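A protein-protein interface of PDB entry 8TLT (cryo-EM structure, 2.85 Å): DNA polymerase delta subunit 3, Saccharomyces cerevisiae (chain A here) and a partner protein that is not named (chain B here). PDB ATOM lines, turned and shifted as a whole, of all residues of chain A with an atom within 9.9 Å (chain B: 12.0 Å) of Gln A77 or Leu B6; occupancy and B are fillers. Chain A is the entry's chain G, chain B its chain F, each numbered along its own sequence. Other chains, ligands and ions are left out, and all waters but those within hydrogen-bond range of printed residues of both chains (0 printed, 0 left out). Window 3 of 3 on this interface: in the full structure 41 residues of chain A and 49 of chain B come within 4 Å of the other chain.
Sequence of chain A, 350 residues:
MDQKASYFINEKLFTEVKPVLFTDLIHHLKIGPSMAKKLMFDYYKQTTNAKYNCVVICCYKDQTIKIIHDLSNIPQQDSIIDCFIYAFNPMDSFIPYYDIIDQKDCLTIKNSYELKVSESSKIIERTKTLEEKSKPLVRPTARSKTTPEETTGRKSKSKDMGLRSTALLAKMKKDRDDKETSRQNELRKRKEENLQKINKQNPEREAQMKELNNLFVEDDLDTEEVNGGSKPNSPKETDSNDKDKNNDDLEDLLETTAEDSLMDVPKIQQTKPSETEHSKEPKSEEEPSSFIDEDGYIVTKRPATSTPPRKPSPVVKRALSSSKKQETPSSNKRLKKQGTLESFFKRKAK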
ATOM      1  N   CYS A  58      14.188  11.918  14.054  1.00  0.00           N
ATOM      2  CA  CYS A  58      15.207  11.232  14.835  1.00  0.00           C
ATOM      3  C   CYS A  58      15.291  11.865  16.215  1.00  0.00           C
ATOM      4  O   CYS A  58      15.413  13.088  16.334  1.00  0.00           O
ATOM      5  CB  CYS A  58      16.566  11.292  14.136  1.00  0.00           C
ATOM      6  SG  CYS A  58      16.776  10.079  12.815  1.00  0.00           S
ATOM      7  N   CYS A  59      15.227  11.032  17.249  1.00  0.00           N
ATOM      8  CA  CYS A  59      15.313  11.484  18.631  1.00  0.00           C
ATOM      9  C   CYS A  59      16.740  11.277  19.123  1.00  0.00           C
ATOM     10  O   CYS A  59      17.246  10.150  19.114  1.00  0.00           O
ATOM     11  CB  CYS A  59      14.322  10.724  19.513  1.00  0.00           C
ATOM     12  SG  CYS A  59      12.590  11.117  19.193  1.00  0.00           S
ATOM     13  N   TYR A  60      17.381  12.359  19.548  1.00  0.00           N
ATOM     14  CA  TYR A  60      18.780  12.331  19.948  1.00  0.00           C
ATOM     15  C   TYR A  60      18.902  12.213  21.464  1.00  0.00           C
ATOM     16  O   TYR A  60      17.918  12.285  22.202  1.00  0.00           O
ATOM     17  CB  TYR A  60      19.505  13.585  19.450  1.00  0.00           C
ATOM     18  CG  TYR A  60      19.880  13.546  17.984  1.00  0.00           C
ATOM     19  CD1 TYR A  60      19.125  12.825  17.072  1.00  0.00           C
ATOM     20  CD2 TYR A  60      20.989  14.235  17.515  1.00  0.00           C
ATOM     21  CE1 TYR A  60      19.462  12.789  15.735  1.00  0.00           C
ATOM     22  CE2 TYR A  60      21.334  14.205  16.178  1.00  0.00           C
ATOM     23  CZ  TYR A  60      20.566  13.479  15.292  1.00  0.00           C
ATOM     24  OH  TYR A  60      20.900  13.441  13.959  1.00  0.00           O
ATOM     25  N   LYS A  61      20.141  12.026  21.922  1.00  0.00           N
ATOM     26  CA  LYS A  61      20.393  11.931  23.356  1.00  0.00           C
ATOM     27  C   LYS A  61      20.111  13.249  24.065  1.00  0.00           C
ATOM     28  O   LYS A  61      19.732  13.250  25.242  1.00  0.00           O
ATOM     29  CB  LYS A  61      21.834  11.489  23.612  1.00  0.00           C
ATOM     30  CG  LYS A  61      22.143  10.078  23.140  1.00  0.00           C
ATOM     31  CD  LYS A  61      23.629   9.895  22.877  1.00  0.00           C
ATOM     32  N   ILE A  68      13.883  14.752   9.437  1.00  0.00           N
ATOM     33  CA  ILE A  68      14.889  14.332   8.467  1.00  0.00           C
ATOM     34  C   ILE A  68      14.464  14.814   7.086  1.00  0.00           C
ATOM     35  O   ILE A  68      13.377  14.478   6.606  1.00  0.00           O
ATOM     36  CB  ILE A  68      15.080  12.810   8.490  1.00  0.00           C
ATOM     37  CG1 ILE A  68      15.481  12.350   9.891  1.00  0.00           C
ATOM     38  CG2 ILE A  68      16.125  12.391   7.473  1.00  0.00           C
ATOM     39  CD1 ILE A  68      16.826  12.866  10.335  1.00  0.00           C
ATOM     40  N   ASP A  70      17.294  15.657   4.319  1.00  0.00           N
ATOM     41  CA  ASP A  70      18.259  15.249   3.303  1.00  0.00           C
ATOM     42  C   ASP A  70      18.080  13.785   2.918  1.00  0.00           C
ATOM     43  O   ASP A  70      18.237  13.422   1.746  1.00  0.00           O
ATOM     44  CB  ASP A  70      19.681  15.504   3.800  1.00  0.00           C
ATOM     45  N   LEU A  71      17.775  12.930   3.894  1.00  0.00           N
ATOM     46  CA  LEU A  71      17.555  11.497   3.713  1.00  0.00           C
ATOM     47  C   LEU A  71      18.796  10.765   3.214  1.00  0.00           C
ATOM     48  O   LEU A  71      18.717   9.578   2.875  1.00  0.00           O
ATOM     49  CB  LEU A  71      16.374  11.225   2.769  1.00  0.00           C
ATOM     50  CG  LEU A  71      15.075  10.716   3.398  1.00  0.00           C
ATOM     51  CD1 LEU A  71      13.919  10.846   2.417  1.00  0.00           C
ATOM     52  CD2 LEU A  71      15.232   9.278   3.862  1.00  0.00           C
ATOM     53  N   SER A  72      19.942  11.440   3.157  1.00  0.00           N
ATOM     54  CA  SER A  72      21.197  10.831   2.738  1.00  0.00           C
ATOM     55  C   SER A  72      22.269  10.915   3.811  1.00  0.00           C
ATOM     56  O   SER A  72      22.946   9.917   4.085  1.00  0.00           O
ATOM     57  CB  SER A  72      21.697  11.490   1.442  1.00  0.00           C
ATOM     58  N   ASN A  73      22.444  12.081   4.430  1.00  0.00           N
ATOM     59  CA  ASN A  73      23.436  12.286   5.479  1.00  0.00           C
ATOM     60  C   ASN A  73      22.716  12.757   6.735  1.00  0.00           C
ATOM     61  O   ASN A  73      22.154  13.858   6.759  1.00  0.00           O
ATOM     62  CB  ASN A  73      24.497  13.296   5.041  1.00  0.00           C
ATOM     63  N   ILE A  74      22.732  11.928   7.773  1.00  0.00           N
ATOM     64  CA  ILE A  74      22.092  12.223   9.049  1.00  0.00           C
ATOM     65  C   ILE A  74      23.196  12.488  10.072  1.00  0.00           C
ATOM     66  O   ILE A  74      23.921  11.557  10.452  1.00  0.00           O
ATOM     67  CB  ILE A  74      21.175  11.080   9.499  1.00  0.00           C
ATOM     68  CG1 ILE A  74      20.368  10.553   8.311  1.00  0.00           C
ATOM     69  CG2 ILE A  74      20.256  11.541  10.615  1.00  0.00           C
ATOM     70  CD1 ILE A  74      19.354   9.498   8.679  1.00  0.00           C
ATOM     71  N   PRO A  75      23.364  13.723  10.538  1.00  0.00           N
ATOM     72  CA  PRO A  75      24.447  14.008  11.486  1.00  0.00           C
ATOM     73  C   PRO A  75      24.236  13.313  12.821  1.00  0.00           C
ATOM     74  O   PRO A  75      23.105  13.085  13.260  1.00  0.00           O
ATOM     75  CB  PRO A  75      24.390  15.532  11.640  1.00  0.00           C
ATOM     76  N   GLN A  76      25.354  12.979  13.467  1.00  0.00           N
ATOM     77  CA  GLN A  76      25.365  12.332  14.779  1.00  0.00           C
ATOM     78  C   GLN A  76      24.548  11.039  14.761  1.00  0.00           C
ATOM     79  O   GLN A  76      23.547  10.888  15.464  1.00  0.00           O
ATOM     80  CB  GLN A  76      24.864  13.291  15.865  1.00  0.00           C
ATOM     81  N   GLN A  77      25.002  10.097  13.929  1.00  0.00           N
ATOM     82  CA  GLN A  77      24.303   8.823  13.800  1.00  0.00           C
ATOM     83  C   GLN A  77      24.333   8.039  15.105  1.00  0.00           C
ATOM     84  O   GLN A  77      23.344   7.395  15.475  1.00  0.00           O
ATOM     85  CB  GLN A  77      24.918   8.003  12.666  1.00  0.00           C
ATOM     86  CG  GLN A  77      24.361   8.327  11.292  1.00  0.00           C
ATOM     87  CD  GLN A  77      23.229   7.404  10.889  1.00  0.00           C
ATOM     88  OE1 GLN A  77      22.861   6.493  11.631  1.00  0.00           O
ATOM     89  NE2 GLN A  77      22.670   7.635   9.708  1.00  0.00           N
ATOM     90  N   ASP A  78      25.462   8.076  15.816  1.00  0.00           N
ATOM     91  CA  ASP A  78      25.569   7.360  17.082  1.00  0.00           C
ATOM     92  C   ASP A  78      24.747   8.007  18.187  1.00  0.00           C
ATOM     93  O   ASP A  78      24.506   7.367  19.217  1.00  0.00           O
ATOM     94  CB  ASP A  78      27.033   7.269  17.512  1.00  0.00           C
ATOM     95  CG  ASP A  78      27.842   8.478  17.084  1.00  0.00           C
ATOM     96  N   SER A  79      24.315   9.254  18.004  1.00  0.00           N
ATOM     97  CA  SER A  79      23.530   9.956  19.010  1.00  0.00           C
ATOM     98  C   SER A  79      22.032   9.714  18.881  1.00  0.00           C
ATOM     99  O   SER A  79      21.276  10.147  19.755  1.00  0.00           O
ATOM    100  CB  SER A  79      23.806  11.461  18.940  1.00  0.00           C
ATOM    101  OG  SER A  79      25.160  11.745  19.244  1.00  0.00           O
ATOM    102  N   ILE A  80      21.588   9.033  17.826  1.00  0.00           N
ATOM    103  CA  ILE A  80      20.163   8.797  17.629  1.00  0.00           C
ATOM    104  C   ILE A  80      19.700   7.722  18.604  1.00  0.00           C
ATOM    105  O   ILE A  80      20.246   6.614  18.636  1.00  0.00           O
ATOM    106  CB  ILE A  80      19.867   8.398  16.179  1.00  0.00           C
ATOM    107  CG1 ILE A  80      20.554   9.362  15.211  1.00  0.00           C
ATOM    108  CG2 ILE A  80      18.370   8.371  15.929  1.00  0.00           C
ATOM    109  N   ILE A  81      18.687   8.047  19.403  1.00  0.00           N
ATOM    110  CA  ILE A  81      18.138   7.107  20.369  1.00  0.00           C
ATOM    111  C   ILE A  81      16.787   6.547  19.940  1.00  0.00           C
ATOM    112  O   ILE A  81      16.344   5.539  20.513  1.00  0.00           O
ATOM    113  CB  ILE A  81      18.032   7.748  21.770  1.00  0.00           C
ATOM    114  CG1 ILE A  81      18.221   6.689  22.859  1.00  0.00           C
ATOM    115  CG2 ILE A  81      16.705   8.472  21.937  1.00  0.00           C
ATOM    116  N   ASP A  82      16.124   7.152  18.958  1.00  0.00           N
ATOM    117  CA  ASP A  82      14.858   6.646  18.450  1.00  0.00           C
ATOM    118  C   ASP A  82      14.643   7.201  17.051  1.00  0.00           C
ATOM    119  O   ASP A  82      15.006   8.345  16.771  1.00  0.00           O
ATOM    120  CB  ASP A  82      13.689   7.029  19.363  1.00  0.00           C
ATOM    121  N   CYS A  83      14.059   6.383  16.180  1.00  0.00           N
ATOM    122  CA  CYS A  83      13.778   6.791  14.811  1.00  0.00           C
ATOM    123  C   CYS A  83      12.508   6.090  14.354  1.00  0.00           C
ATOM    124  O   CYS A  83      12.398   4.867  14.479  1.00  0.00           O
ATOM    125  CB  CYS A  83      14.947   6.450  13.881  1.00  0.00           C
ATOM    126  SG  CYS A  83      14.786   7.099  12.206  1.00  0.00           S
ATOM    127  N   LEU B   6      24.758   5.953   5.890  1.00  0.00           N
ATOM    128  CA  LEU B   6      23.853   4.987   6.501  1.00  0.00           C
ATOM    129  C   LEU B   6      22.428   5.271   6.036  1.00  0.00           C
ATOM    130  O   LEU B   6      21.864   6.321   6.342  1.00  0.00           O
ATOM    131  CB  LEU B   6      23.963   5.045   8.031  1.00  0.00           C
ATOM    132  CG  LEU B   6      23.537   3.848   8.891  1.00  0.00           C
ATOM    133  CD1 LEU B   6      22.042   3.579   8.837  1.00  0.00           C
ATOM    134  CD2 LEU B   6      24.317   2.604   8.489  1.00  0.00           C
ATOM    135  N   HIS B   7      21.856   4.328   5.291  1.00  0.00           N
ATOM    136  CA  HIS B   7      20.533   4.514   4.711  1.00  0.00           C
ATOM    137  C   HIS B   7      19.465   4.596   5.796  1.00  0.00           C
ATOM    138  O   HIS B   7      19.548   3.935   6.835  1.00  0.00           O
ATOM    139  CB  HIS B   7      20.210   3.374   3.748  1.00  0.00           C
ATOM    140  N   MET B   8      18.445   5.420   5.538  1.00  0.00           N
ATOM    141  CA  MET B   8      17.370   5.592   6.510  1.00  0.00           C
ATOM    142  C   MET B   8      16.569   4.311   6.699  1.00  0.00           C
ATOM    143  O   MET B   8      15.966   4.111   7.760  1.00  0.00           O
ATOM    144  CB  MET B   8      16.449   6.734   6.083  1.00  0.00           C
ATOM    145  CG  MET B   8      15.842   7.506   7.242  1.00  0.00           C
ATOM    146  N   ASP B   9      16.536   3.441   5.687  1.00  0.00           N
ATOM    147  CA  ASP B   9      15.866   2.155   5.849  1.00  0.00           C
ATOM    148  C   ASP B   9      16.547   1.317   6.922  1.00  0.00           C
ATOM    149  O   ASP B   9      15.878   0.636   7.709  1.00  0.00           O
ATOM    150  CB  ASP B   9      15.838   1.403   4.518  1.00  0.00           C
ATOM    151  CG  ASP B   9      14.849   1.995   3.535  1.00  0.00           C
ATOM    152  N   ALA B  10      17.882   1.353   6.967  1.00  0.00           N
ATOM    153  CA  ALA B  10      18.608   0.620   7.998  1.00  0.00           C
ATOM    154  C   ALA B  10      18.282   1.151   9.388  1.00  0.00           C
ATOM    155  O   ALA B  10      18.082   0.372  10.325  1.00  0.00           O
ATOM    156  CB  ALA B  10      20.111   0.692   7.733  1.00  0.00           C
ATOM    157  N   LEU B  11      18.219   2.475   9.544  1.00  0.00           N
ATOM    158  CA  LEU B  11      17.862   3.047  10.840  1.00  0.00           C
ATOM    159  C   LEU B  11      16.432   2.690  11.228  1.00  0.00           C
ATOM    160  O   LEU B  11      16.154   2.381  12.394  1.00  0.00           O
ATOM    161  CB  LEU B  11      18.052   4.562  10.814  1.00  0.00           C
ATOM    162  CG  LEU B  11      19.463   5.061  11.127  1.00  0.00           C
ATOM    163  CD1 LEU B  11      19.565   6.560  10.905  1.00  0.00           C
ATOM    164  CD2 LEU B  11      19.855   4.697  12.549  1.00  0.00           C
ATOM    165  N   LEU B  12      15.512   2.731  10.262  1.00  0.00           N
ATOM    166  CA  LEU B  12      14.125   2.376  10.542  1.00  0.00           C
ATOM    167  C   LEU B  12      14.006   0.923  10.983  1.00  0.00           C
ATOM    168  O   LEU B  12      13.311   0.620  11.958  1.00  0.00           O
ATOM    169  CB  LEU B  12      13.260   2.636   9.308  1.00  0.00           C
ATOM    170  CG  LEU B  12      12.318   3.841   9.355  1.00  0.00           C
ATOM    171  CD1 LEU B  12      13.069   5.099   9.745  1.00  0.00           C
ATOM    172  CD2 LEU B  12      11.630   4.028   8.016  1.00  0.00           C
ATOM    173  N   THR B  13      14.689   0.011  10.290  1.00  0.00           N
ATOM    174  CA  THR B  13      14.639  -1.396  10.659  1.00  0.00           C
ATOM    175  C   THR B  13      15.488  -1.718  11.883  1.00  0.00           C
ATOM    176  O   THR B  13      15.349  -2.810  12.443  1.00  0.00           O
ATOM    177  CB  THR B  13      15.077  -2.274   9.481  1.00  0.00           C
ATOM    178  OG1 THR B  13      14.644  -3.622   9.700  1.00  0.00           O
ATOM    179  CG2 THR B  13      16.588  -2.255   9.327  1.00  0.00           C
ATOM    180  N   LYS B  14      16.364  -0.806  12.302  1.00  0.00           N
ATOM    181  CA  LYS B  14      17.133  -0.993  13.524  1.00  0.00           C
ATOM    182  C   LYS B  14      16.397  -0.486  14.756  1.00  0.00           C
ATOM    183  O   LYS B  14      16.581  -1.035  15.849  1.00  0.00           O
ATOM    184  CB  LYS B  14      18.486  -0.287  13.396  1.00  0.00           C
ATOM    185  CG  LYS B  14      19.388  -0.388  14.616  1.00  0.00           C
ATOM    186  CD  LYS B  14      19.481   0.937  15.352  1.00  0.00           C
ATOM    187  CE  LYS B  14      20.419   0.841  16.543  1.00  0.00           C
ATOM    188  N   PHE B  15      15.559   0.539  14.605  1.00  0.00           N
ATOM    189  CA  PHE B  15      14.836   1.115  15.732  1.00  0.00           C
ATOM    190  C   PHE B  15      13.394   0.642  15.831  1.00  0.00           C
ATOM    191  O   PHE B  15      12.977   0.153  16.885  1.00  0.00           O
ATOM    192  CB  PHE B  15      14.877   2.647  15.651  1.00  0.00           C
ATOM    193  CG  PHE B  15      16.153   3.242  16.165  1.00  0.00           C
ATOM    194  CD1 PHE B  15      16.435   3.242  17.520  1.00  0.00           C
ATOM    195  CD2 PHE B  15      17.076   3.795  15.295  1.00  0.00           C
ATOM    196  CE1 PHE B  15      17.609   3.787  17.997  1.00  0.00           C
ATOM    197  CE2 PHE B  15      18.253   4.340  15.765  1.00  0.00           C
ATOM    198  CZ  PHE B  15      18.520   4.336  17.119  1.00  0.00           C
ATOM    199  N   ASN B  16      12.612   0.773  14.759  1.00  0.00           N
ATOM    200  CA  ASN B  16      11.190   0.461  14.824  1.00  0.00           C
ATOM    201  C   ASN B  16      10.899  -1.035  14.840  1.00  0.00           C
ATOM    202  O   ASN B  16       9.839  -1.435  15.330  1.00  0.00           O
ATOM    203  CB  ASN B  16      10.460   1.109  13.648  1.00  0.00           C
ATOM    204  CG  ASN B  16      10.375   2.616  13.776  1.00  0.00           C
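CB of Met B8 touches CD2 of Leu A71 (3.6 Å).
CD1 of Leu B11 touches CD1 of Ile A74, at 3.7 Å.
Gln A77 touches Leu B6 (NE2 to CB, 3.3 Å).
Leu B11 touches Gln A77.
O of Ile A80 touches CZ of Phe B15, 3.2 Å away.
O of Ile A81 touches CE1 of Phe B15, 3.3 Å away.
Asp A82 touches Phe B15.
Leu B12 touches Cys A83.
CB of Phe B15 touches O of Cys A83 (3.5 Å).
Asn B16 touches Cys A83.
Gln A77 touches just these residues of chain B: Leu B6 and Leu B11.
Leu B6 touches just one residue of chain A: Gln A77 (3.3 Å).
No residue of chain B comes within 4 Å of Ser A72.
No residue of chain B comes within 4 Å of Asn A73.
No residue of chain B comes within 4 Å of Gln A76.
No residue of chain B comes within 4 Å of Asp A78.
No residue of chain A comes within 4 Å of Ala B10.
Of the printed residues of chain B, Ile A81 touches Phe B15.
Printed residues of chain A within 4 Å of Met B8: Leu A71 (3.6 Å).
The nearest printed residue of chain A that does not touch Leu B11 is Cys A83 (4.4 Å).
SG of Cys A58 sits at hydrogen-bond distance from SG of Cys A83.
The backbone carbonyl oxygen of Cys A59 sits at hydrogen-bond distance from the backbone NH of Ile A81, at 2.6 Å.
The backbone NH of Cys A59 lies within hydrogen-bond range of the backbone carbonyl oxygen of Asp A82 (2.7 Å).
Of the 19 printed residues of chain A, 7 touch a printed residue of chain B.
Printed residues of chain A that touch a printed residue of chain B: Leu A71, Ile A74, Gln A77, Ile A80, Ile A81, Asp A82 and Cys A83.
Among the printed residues, 10 pairs touch across the chains.
Among the printed residues, no Asp or Glu carboxylate lies within 4 Å of a Lys or Arg side-chain nitrogen of the other chain.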
